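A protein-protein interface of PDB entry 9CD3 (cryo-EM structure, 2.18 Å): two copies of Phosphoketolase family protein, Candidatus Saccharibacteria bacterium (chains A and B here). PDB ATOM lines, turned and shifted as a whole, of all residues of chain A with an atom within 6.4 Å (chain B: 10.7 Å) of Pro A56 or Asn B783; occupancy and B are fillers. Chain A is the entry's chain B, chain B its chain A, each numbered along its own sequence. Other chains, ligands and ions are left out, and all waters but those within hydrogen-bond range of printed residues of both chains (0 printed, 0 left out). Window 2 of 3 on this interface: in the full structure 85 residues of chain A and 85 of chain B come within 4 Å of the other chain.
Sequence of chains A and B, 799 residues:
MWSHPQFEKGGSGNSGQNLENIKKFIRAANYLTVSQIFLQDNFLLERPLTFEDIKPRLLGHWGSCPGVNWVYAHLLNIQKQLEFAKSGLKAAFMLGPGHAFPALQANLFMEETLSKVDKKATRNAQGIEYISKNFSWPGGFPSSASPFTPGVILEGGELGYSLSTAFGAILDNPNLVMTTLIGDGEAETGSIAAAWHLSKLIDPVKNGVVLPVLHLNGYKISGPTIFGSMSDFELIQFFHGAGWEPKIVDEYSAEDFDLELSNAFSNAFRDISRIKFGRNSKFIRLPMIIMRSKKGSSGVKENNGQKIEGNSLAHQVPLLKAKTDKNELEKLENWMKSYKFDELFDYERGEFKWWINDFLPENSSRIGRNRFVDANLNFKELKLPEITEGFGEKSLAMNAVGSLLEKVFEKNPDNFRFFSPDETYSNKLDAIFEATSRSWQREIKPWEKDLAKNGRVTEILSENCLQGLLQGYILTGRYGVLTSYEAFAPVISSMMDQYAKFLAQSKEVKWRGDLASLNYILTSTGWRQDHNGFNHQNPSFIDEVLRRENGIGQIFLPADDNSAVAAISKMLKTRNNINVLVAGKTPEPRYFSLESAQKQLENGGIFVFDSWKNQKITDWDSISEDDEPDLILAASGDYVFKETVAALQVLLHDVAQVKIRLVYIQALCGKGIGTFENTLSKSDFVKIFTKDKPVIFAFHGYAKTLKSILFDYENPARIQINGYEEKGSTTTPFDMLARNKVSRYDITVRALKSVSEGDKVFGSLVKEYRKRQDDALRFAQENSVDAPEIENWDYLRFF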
ATOM      1  N   GLN A  40     -28.344  16.068  20.916  1.00  0.00           N
ATOM      2  CA  GLN A  40     -27.880  14.730  21.247  1.00  0.00           C
ATOM      3  C   GLN A  40     -27.569  14.571  22.729  1.00  0.00           C
ATOM      4  O   GLN A  40     -27.483  13.437  23.214  1.00  0.00           O
ATOM      5  CB  GLN A  40     -26.623  14.398  20.433  1.00  0.00           C
ATOM      6  CG  GLN A  40     -26.331  12.923  20.266  1.00  0.00           C
ATOM      7  CD  GLN A  40     -24.956  12.674  19.680  1.00  0.00           C
ATOM      8  OE1 GLN A  40     -24.163  13.599  19.515  1.00  0.00           O
ATOM      9  NE2 GLN A  40     -24.668  11.421  19.359  1.00  0.00           N
ATOM     10  N   ILE A  54     -24.743  18.034  19.282  1.00  0.00           N
ATOM     11  CA  ILE A  54     -25.557  18.138  18.078  1.00  0.00           C
ATOM     12  C   ILE A  54     -25.516  16.800  17.356  1.00  0.00           C
ATOM     13  O   ILE A  54     -24.476  16.133  17.328  1.00  0.00           O
ATOM     14  CB  ILE A  54     -25.070  19.276  17.156  1.00  0.00           C
ATOM     15  CG1 ILE A  54     -24.725  20.519  17.978  1.00  0.00           C
ATOM     16  CG2 ILE A  54     -26.122  19.608  16.109  1.00  0.00           C
ATOM     17  CD1 ILE A  54     -25.926  21.242  18.525  1.00  0.00           C
ATOM     18  N   LYS A  55     -26.649  16.403  16.786  1.00  0.00           N
ATOM     19  CA  LYS A  55     -26.732  15.109  16.124  1.00  0.00           C
ATOM     20  C   LYS A  55     -25.842  15.090  14.883  1.00  0.00           C
ATOM     21  O   LYS A  55     -25.695  16.115  14.207  1.00  0.00           O
ATOM     22  CB  LYS A  55     -28.176  14.796  15.734  1.00  0.00           C
ATOM     23  CG  LYS A  55     -29.046  14.322  16.881  1.00  0.00           C
ATOM     24  CD  LYS A  55     -30.490  14.175  16.441  1.00  0.00           C
ATOM     25  CE  LYS A  55     -31.367  13.678  17.573  1.00  0.00           C
ATOM     26  NZ  LYS A  55     -32.592  14.506  17.702  1.00  0.00           N
ATOM     27  N   PRO A  56     -25.231  13.947  14.558  1.00  0.00           N
ATOM     28  CA  PRO A  56     -24.403  13.879  13.344  1.00  0.00           C
ATOM     29  C   PRO A  56     -25.173  14.161  12.067  1.00  0.00           C
ATOM     30  O   PRO A  56     -24.611  14.739  11.130  1.00  0.00           O
ATOM     31  CB  PRO A  56     -23.860  12.443  13.369  1.00  0.00           C
ATOM     32  CG  PRO A  56     -24.052  11.974  14.775  1.00  0.00           C
ATOM     33  CD  PRO A  56     -25.275  12.663  15.271  1.00  0.00           C
ATOM     34  N   ARG A  57     -26.441  13.764  11.994  1.00  0.00           N
ATOM     35  CA  ARG A  57     -27.298  14.065  10.855  1.00  0.00           C
ATOM     36  C   ARG A  57     -28.562  14.737  11.359  1.00  0.00           C
ATOM     37  O   ARG A  57     -29.261  14.187  12.215  1.00  0.00           O
ATOM     38  CB  ARG A  57     -27.663  12.804  10.069  1.00  0.00           C
ATOM     39  CG  ARG A  57     -26.486  12.010   9.547  1.00  0.00           C
ATOM     40  CD  ARG A  57     -26.975  10.826   8.737  1.00  0.00           C
ATOM     41  NE  ARG A  57     -28.179  10.242   9.318  1.00  0.00           N
ATOM     42  CZ  ARG A  57     -28.531   8.969   9.193  1.00  0.00           C
ATOM     43  NH1 ARG A  57     -27.795   8.113   8.507  1.00  0.00           N
ATOM     44  NH2 ARG A  57     -29.650   8.548   9.775  1.00  0.00           N
ATOM     45  N   LEU A  58     -28.859  15.914  10.826  1.00  0.00           N
ATOM     46  CA  LEU A  58     -30.058  16.652  11.193  1.00  0.00           C
ATOM     47  C   LEU A  58     -31.168  16.299  10.214  1.00  0.00           C
ATOM     48  O   LEU A  58     -31.025  16.506   9.004  1.00  0.00           O
ATOM     49  CB  LEU A  58     -29.796  18.158  11.201  1.00  0.00           C
ATOM     50  CG  LEU A  58     -28.655  18.607  12.114  1.00  0.00           C
ATOM     51  CD1 LEU A  58     -28.528  20.121  12.117  1.00  0.00           C
ATOM     52  CD2 LEU A  58     -28.862  18.080  13.523  1.00  0.00           C
ATOM     53  N   TRP A 137     -33.737   8.666  15.048  1.00  0.00           N
ATOM     54  CA  TRP A 137     -32.572   7.815  15.243  1.00  0.00           C
ATOM     55  C   TRP A 137     -32.828   6.432  14.649  1.00  0.00           C
ATOM     56  O   TRP A 137     -33.963   5.950  14.669  1.00  0.00           O
ATOM     57  CB  TRP A 137     -32.244   7.690  16.731  1.00  0.00           C
ATOM     58  CG  TRP A 137     -30.843   7.239  17.024  1.00  0.00           C
ATOM     59  CD1 TRP A 137     -30.397   5.952  17.108  1.00  0.00           C
ATOM     60  CD2 TRP A 137     -29.709   8.073  17.285  1.00  0.00           C
ATOM     61  NE1 TRP A 137     -29.056   5.933  17.398  1.00  0.00           N
ATOM     62  CE2 TRP A 137     -28.609   7.222  17.512  1.00  0.00           C
ATOM     63  CE3 TRP A 137     -29.516   9.455  17.346  1.00  0.00           C
ATOM     64  CZ2 TRP A 137     -27.337   7.710  17.795  1.00  0.00           C
ATOM     65  CZ3 TRP A 137     -28.252   9.935  17.626  1.00  0.00           C
ATOM     66  CH2 TRP A 137     -27.178   9.066  17.847  1.00  0.00           C
ATOM     67  N   PRO A 138     -31.803   5.783  14.097  1.00  0.00           N
ATOM     68  CA  PRO A 138     -31.969   4.395  13.642  1.00  0.00           C
ATOM     69  C   PRO A 138     -32.335   3.486  14.806  1.00  0.00           C
ATOM     70  O   PRO A 138     -31.596   3.371  15.785  1.00  0.00           O
ATOM     71  CB  PRO A 138     -30.596   4.049  13.057  1.00  0.00           C
ATOM     72  CG  PRO A 138     -29.996   5.362  12.698  1.00  0.00           C
ATOM     73  CD  PRO A 138     -30.493   6.337  13.720  1.00  0.00           C
ATOM     74  N   LYS A 323     -23.383  22.008  13.702  1.00  0.00           N
ATOM     75  CA  LYS A 323     -22.313  21.202  14.274  1.00  0.00           C
ATOM     76  C   LYS A 323     -20.934  21.585  13.751  1.00  0.00           C
ATOM     77  O   LYS A 323     -19.932  21.055  14.246  1.00  0.00           O
ATOM     78  CB  LYS A 323     -22.573  19.718  14.002  1.00  0.00           C
ATOM     79  CG  LYS A 323     -21.899  18.782  14.990  1.00  0.00           C
ATOM     80  CD  LYS A 323     -22.157  17.327  14.657  1.00  0.00           C
ATOM     81  CE  LYS A 323     -21.540  16.420  15.703  1.00  0.00           C
ATOM     82  NZ  LYS A 323     -21.733  14.985  15.375  1.00  0.00           N
ATOM     83  N   HIS B 531     -35.233  12.225   5.068  1.00  0.00           N
ATOM     84  CA  HIS B 531     -36.148  12.976   5.915  1.00  0.00           C
ATOM     85  C   HIS B 531     -37.526  12.336   6.022  1.00  0.00           C
ATOM     86  O   HIS B 531     -38.386  12.869   6.733  1.00  0.00           O
ATOM     87  CB  HIS B 531     -36.288  14.412   5.397  1.00  0.00           C
ATOM     88  CG  HIS B 531     -35.034  15.222   5.515  1.00  0.00           C
ATOM     89  ND1 HIS B 531     -34.924  16.307   6.356  1.00  0.00           N
ATOM     90  CD2 HIS B 531     -33.834  15.103   4.897  1.00  0.00           C
ATOM     91  CE1 HIS B 531     -33.712  16.821   6.253  1.00  0.00           C
ATOM     92  NE2 HIS B 531     -33.030  16.109   5.374  1.00  0.00           N
ATOM     93  N   THR B 731     -33.691   5.182   8.599  1.00  0.00           N
ATOM     94  CA  THR B 731     -32.436   4.572   9.031  1.00  0.00           C
ATOM     95  C   THR B 731     -31.351   4.934   8.021  1.00  0.00           C
ATOM     96  O   THR B 731     -31.584   5.710   7.086  1.00  0.00           O
ATOM     97  CB  THR B 731     -32.584   3.057   9.185  1.00  0.00           C
ATOM     98  OG1 THR B 731     -31.318   2.487   9.534  1.00  0.00           O
ATOM     99  CG2 THR B 731     -33.071   2.436   7.886  1.00  0.00           C
ATOM    100  N   THR B 732     -30.160   4.372   8.214  1.00  0.00           N
ATOM    101  CA  THR B 732     -29.019   4.633   7.351  1.00  0.00           C
ATOM    102  C   THR B 732     -29.176   3.920   6.011  1.00  0.00           C
ATOM    103  O   THR B 732     -29.891   2.921   5.909  1.00  0.00           O
ATOM    104  CB  THR B 732     -27.731   4.179   8.033  1.00  0.00           C
ATOM    105  OG1 THR B 732     -27.767   2.761   8.233  1.00  0.00           O
ATOM    106  CG2 THR B 732     -27.567   4.873   9.375  1.00  0.00           C
ATOM    107  N   ASP B 774     -23.417  -7.849  10.520  1.00  0.00           N
ATOM    108  CA  ASP B 774     -23.849  -7.614  11.894  1.00  0.00           C
ATOM    109  C   ASP B 774     -23.089  -6.453  12.523  1.00  0.00           C
ATOM    110  O   ASP B 774     -23.686  -5.594  13.182  1.00  0.00           O
ATOM    111  CB  ASP B 774     -23.665  -8.883  12.726  1.00  0.00           C
ATOM    112  CG  ASP B 774     -24.533 -10.026  12.247  1.00  0.00           C
ATOM    113  OD1 ASP B 774     -25.156  -9.891  11.174  1.00  0.00           O
ATOM    114  OD2 ASP B 774     -24.590 -11.061  12.943  1.00  0.00           O
ATOM    115  N   ASP B 775     -21.768  -6.413  12.329  1.00  0.00           N
ATOM    116  CA  ASP B 775     -20.960  -5.332  12.878  1.00  0.00           C
ATOM    117  C   ASP B 775     -21.356  -3.993  12.277  1.00  0.00           C
ATOM    118  O   ASP B 775     -21.446  -2.986  12.989  1.00  0.00           O
ATOM    119  CB  ASP B 775     -19.478  -5.607  12.630  1.00  0.00           C
ATOM    120  CG  ASP B 775     -18.952  -6.772  13.444  1.00  0.00           C
ATOM    121  OD1 ASP B 775     -19.659  -7.228  14.366  1.00  0.00           O
ATOM    122  OD2 ASP B 775     -17.827  -7.231  13.161  1.00  0.00           O
ATOM    123  N   ALA B 776     -21.590  -3.959  10.963  1.00  0.00           N
ATOM    124  CA  ALA B 776     -21.993  -2.713  10.320  1.00  0.00           C
ATOM    125  C   ALA B 776     -23.333  -2.224  10.854  1.00  0.00           C
ATOM    126  O   ALA B 776     -23.501  -1.029  11.133  1.00  0.00           O
ATOM    127  CB  ALA B 776     -22.053  -2.903   8.806  1.00  0.00           C
ATOM    128  N   LEU B 777     -24.300  -3.132  11.011  1.00  0.00           N
ATOM    129  CA  LEU B 777     -25.603  -2.732  11.535  1.00  0.00           C
ATOM    130  C   LEU B 777     -25.498  -2.257  12.980  1.00  0.00           C
ATOM    131  O   LEU B 777     -26.162  -1.290  13.372  1.00  0.00           O
ATOM    132  CB  LEU B 777     -26.598  -3.886  11.413  1.00  0.00           C
ATOM    133  CG  LEU B 777     -26.896  -4.359   9.990  1.00  0.00           C
ATOM    134  CD1 LEU B 777     -27.777  -5.597  10.000  1.00  0.00           C
ATOM    135  CD2 LEU B 777     -27.533  -3.248   9.175  1.00  0.00           C
ATOM    136  N   ARG B 778     -24.671  -2.926  13.788  1.00  0.00           N
ATOM    137  CA  ARG B 778     -24.474  -2.491  15.168  1.00  0.00           C
ATOM    138  C   ARG B 778     -23.837  -1.108  15.226  1.00  0.00           C
ATOM    139  O   ARG B 778     -24.244  -0.260  16.031  1.00  0.00           O
ATOM    140  CB  ARG B 778     -23.613  -3.505  15.917  1.00  0.00           C
ATOM    141  CG  ARG B 778     -24.366  -4.312  16.957  1.00  0.00           C
ATOM    142  CD  ARG B 778     -23.419  -4.863  18.008  1.00  0.00           C
ATOM    143  NE  ARG B 778     -22.236  -5.470  17.411  1.00  0.00           N
ATOM    144  CZ  ARG B 778     -22.201  -6.690  16.892  1.00  0.00           C
ATOM    145  NH1 ARG B 778     -23.272  -7.465  16.876  1.00  0.00           N
ATOM    146  NH2 ARG B 778     -21.063  -7.141  16.374  1.00  0.00           N
ATOM    147  N   PHE B 779     -22.830  -0.865  14.383  1.00  0.00           N
ATOM    148  CA  PHE B 779     -22.200   0.450  14.342  1.00  0.00           C
ATOM    149  C   PHE B 779     -23.204   1.518  13.940  1.00  0.00           C
ATOM    150  O   PHE B 779     -23.231   2.608  14.526  1.00  0.00           O
ATOM    151  CB  PHE B 779     -21.013   0.436  13.377  1.00  0.00           C
ATOM    152  CG  PHE B 779     -20.125   1.644  13.488  1.00  0.00           C
ATOM    153  CD1 PHE B 779     -20.489   2.850  12.911  1.00  0.00           C
ATOM    154  CD2 PHE B 779     -18.926   1.573  14.174  1.00  0.00           C
ATOM    155  CE1 PHE B 779     -19.677   3.960  13.018  1.00  0.00           C
ATOM    156  CE2 PHE B 779     -18.108   2.680  14.281  1.00  0.00           C
ATOM    157  CZ  PHE B 779     -18.484   3.874  13.702  1.00  0.00           C
ATOM    158  N   ALA B 780     -24.033   1.228  12.935  1.00  0.00           N
ATOM    159  CA  ALA B 780     -25.064   2.178  12.534  1.00  0.00           C
ATOM    160  C   ALA B 780     -26.010   2.471  13.691  1.00  0.00           C
ATOM    161  O   ALA B 780     -26.280   3.635  14.005  1.00  0.00           O
ATOM    162  CB  ALA B 780     -25.829   1.643  11.327  1.00  0.00           C
ATOM    163  N   GLN B 781     -26.485   1.420  14.366  1.00  0.00           N
ATOM    164  CA  GLN B 781     -27.411   1.605  15.479  1.00  0.00           C
ATOM    165  C   GLN B 781     -26.792   2.449  16.585  1.00  0.00           C
ATOM    166  O   GLN B 781     -27.474   3.276  17.201  1.00  0.00           O
ATOM    167  CB  GLN B 781     -27.845   0.249  16.033  1.00  0.00           C
ATOM    168  CG  GLN B 781     -29.148  -0.277  15.464  1.00  0.00           C
ATOM    169  CD  GLN B 781     -29.257  -1.784  15.566  1.00  0.00           C
ATOM    170  OE1 GLN B 781     -28.893  -2.375  16.582  1.00  0.00           O
ATOM    171  NE2 GLN B 781     -29.761  -2.415  14.513  1.00  0.00           N
ATOM    172  N   GLU B 782     -25.503   2.252  16.854  1.00  0.00           N
ATOM    173  CA  GLU B 782     -24.866   2.984  17.942  1.00  0.00           C
ATOM    174  C   GLU B 782     -24.564   4.432  17.569  1.00  0.00           C
ATOM    175  O   GLU B 782     -24.656   5.321  18.421  1.00  0.00           O
ATOM    176  CB  GLU B 782     -23.581   2.278  18.372  1.00  0.00           C
ATOM    177  CG  GLU B 782     -23.798   1.115  19.321  1.00  0.00           C
ATOM    178  CD  GLU B 782     -22.672   0.103  19.265  1.00  0.00           C
ATOM    179  OE1 GLU B 782     -21.707   0.329  18.504  1.00  0.00           O
ATOM    180  OE2 GLU B 782     -22.752  -0.918  19.978  1.00  0.00           O
ATOM    181  N   ASN B 783     -24.204   4.698  16.308  1.00  0.00           N
ATOM    182  CA  ASN B 783     -23.603   5.978  15.963  1.00  0.00           C
ATOM    183  C   ASN B 783     -24.434   6.871  15.052  1.00  0.00           C
ATOM    184  O   ASN B 783     -24.031   8.016  14.829  1.00  0.00           O
ATOM    185  CB  ASN B 783     -22.234   5.757  15.305  1.00  0.00           C
ATOM    186  CG  ASN B 783     -21.225   5.145  16.252  1.00  0.00           C
ATOM    187  OD1 ASN B 783     -20.631   5.838  17.074  1.00  0.00           O
ATOM    188  ND2 ASN B 783     -21.026   3.839  16.141  1.00  0.00           N
ATOM    189  N   SER B 784     -25.560   6.395  14.515  1.00  0.00           N
ATOM    190  CA  SER B 784     -26.412   7.147  13.595  1.00  0.00           C
ATOM    191  C   SER B 784     -25.720   7.475  12.278  1.00  0.00           C
ATOM    192  O   SER B 784     -26.229   8.300  11.510  1.00  0.00           O
ATOM    193  CB  SER B 784     -26.942   8.439  14.228  1.00  0.00           C
ATOM    194  OG  SER B 784     -27.797   9.127  13.334  1.00  0.00           O
ATOM    195  N   VAL B 785     -24.570   6.857  11.993  1.00  0.00           N
ATOM    196  CA  VAL B 785     -23.881   7.002  10.717  1.00  0.00           C
ATOM    197  C   VAL B 785     -23.374   5.632  10.289  1.00  0.00           C
ATOM    198  O   VAL B 785     -23.274   4.702  11.092  1.00  0.00           O
ATOM    199  CB  VAL B 785     -22.704   8.002  10.779  1.00  0.00           C
ATOM    200  CG1 VAL B 785     -23.209   9.417  11.019  1.00  0.00           C
ATOM    201  CG2 VAL B 785     -21.715   7.590  11.854  1.00  0.00           C
ATOM    202  N   ASP B 786     -23.048   5.515   9.005  1.00  0.00           N
ATOM    203  CA  ASP B 786     -22.539   4.262   8.472  1.00  0.00           C
ATOM    204  C   ASP B 786     -21.082   4.054   8.869  1.00  0.00           C
ATOM    205  O   ASP B 786     -20.359   5.002   9.188  1.00  0.00           O
ATOM    206  CB  ASP B 786     -22.673   4.225   6.950  1.00  0.00           C
ATOM    207  CG  ASP B 786     -23.911   3.477   6.492  1.00  0.00           C
ATOM    208  OD1 ASP B 786     -24.621   2.915   7.351  1.00  0.00           O
ATOM    209  OD2 ASP B 786     -24.173   3.450   5.272  1.00  0.00           O
ATOM    210  N   ALA B 787     -20.660   2.793   8.847  1.00  0.00           N
ATOM    211  CA  ALA B 787     -19.309   2.444   9.254  1.00  0.00           C
ATOM    212  C   ALA B 787     -18.286   3.003   8.265  1.00  0.00           C
ATOM    213  O   ALA B 787     -18.571   3.135   7.069  1.00  0.00           O
ATOM    214  CB  ALA B 787     -19.163   0.927   9.359  1.00  0.00           C
ATOM    215  N   PRO B 788     -17.087   3.352   8.741  1.00  0.00           N
ATOM    216  CA  PRO B 788     -16.057   3.868   7.825  1.00  0.00           C
ATOM    217  C   PRO B 788     -15.646   2.878   6.752  1.00  0.00           C
ATOM    218  O   PRO B 788     -15.303   3.295   5.639  1.00  0.00           O
ATOM    219  CB  PRO B 788     -14.892   4.202   8.767  1.00  0.00           C
ATOM    220  CG  PRO B 788     -15.110   3.341   9.960  1.00  0.00           C
ATOM    221  CD  PRO B 788     -16.595   3.252  10.126  1.00  0.00           C
ATOM    222  N   GLU B 791     -18.204   3.452   4.187  1.00  0.00           N
ATOM    223  CA  GLU B 791     -18.240   4.835   3.720  1.00  0.00           C
ATOM    224  C   GLU B 791     -17.061   5.155   2.807  1.00  0.00           C
ATOM    225  O   GLU B 791     -17.220   5.873   1.813  1.00  0.00           O
ATOM    226  CB  GLU B 791     -18.267   5.791   4.911  1.00  0.00           C
ATOM    227  CG  GLU B 791     -19.639   5.961   5.532  1.00  0.00           C
ATOM    228  CD  GLU B 791     -20.327   7.234   5.084  1.00  0.00           C
ATOM    229  OE1 GLU B 791     -20.418   7.463   3.861  1.00  0.00           O
ATOM    230  OE2 GLU B 791     -20.779   8.007   5.956  1.00  0.00           O
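O of Ser B784 lies close to NH1 of Arg A57, 3.4 Å away. The indole nitrogen of Trp A137 lies within hydrogen-bond range of the backbone carbonyl oxygen of Gln B781 (3.1 Å).
The side-chain hydroxyl (OG1) of Thr B732 is in hydrogen-bond range of the side-chain carboxylate (OD1) of Asp B786, 3.3 Å away. The backbone carbonyl oxygen (O) of Phe B779 sits at hydrogen-bond distance from the side-chain amide nitrogen (ND2) of Asn B783 (3.0 Å).
Among the printed residues, pairs that only touch across the chains: Pro A56 with Asn B783 (3.96 Å), Pro A56 with Val B785 (3.9 Å), Arg A57 with Thr B732 (3.4 Å), Leu A58 with His B531 (3.9 Å), Trp A137 with Glu B782 (3.6 Å), Trp A137 with Ser B784 (3.7 Å), Pro A138 with Thr B731 (3.9 Å) and Pro A138 with Ser B784 (3.9 Å).
Pro A56 touches just these residues of chain B: Asn B783 and Val B785. Of the printed residues of chain B, Pro A138 touches Thr B731 and Ser B784. Of the printed residues of chain A, Thr B731 touches Pro A138. Printed residues of chain A within 4 Å of Thr B732: Arg A57. Of the printed residues of chain A, Glu B782 touches Trp A137 (3.6 Å). Printed residues of chain A within 4 Å of Asn B783: Pro A56. The nearest printed residue of chain A that does not touch Thr B731 is Arg A57 (4.4 Å).
Along chain A the printed residues that touch a printed residue of chain B span positions 56 to 138. Hydrophobic or aromatic side chains of chain B within 4 Å of the printed part of chain A: His B531 and Val B785. Along chain B the printed residues that touch a printed residue of chain A span positions 531 to 785.
No position is printed for both chains. Of the 10 pairs that touch across the chains among the printed residues, none has its exchanged pair printed and touching as well.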
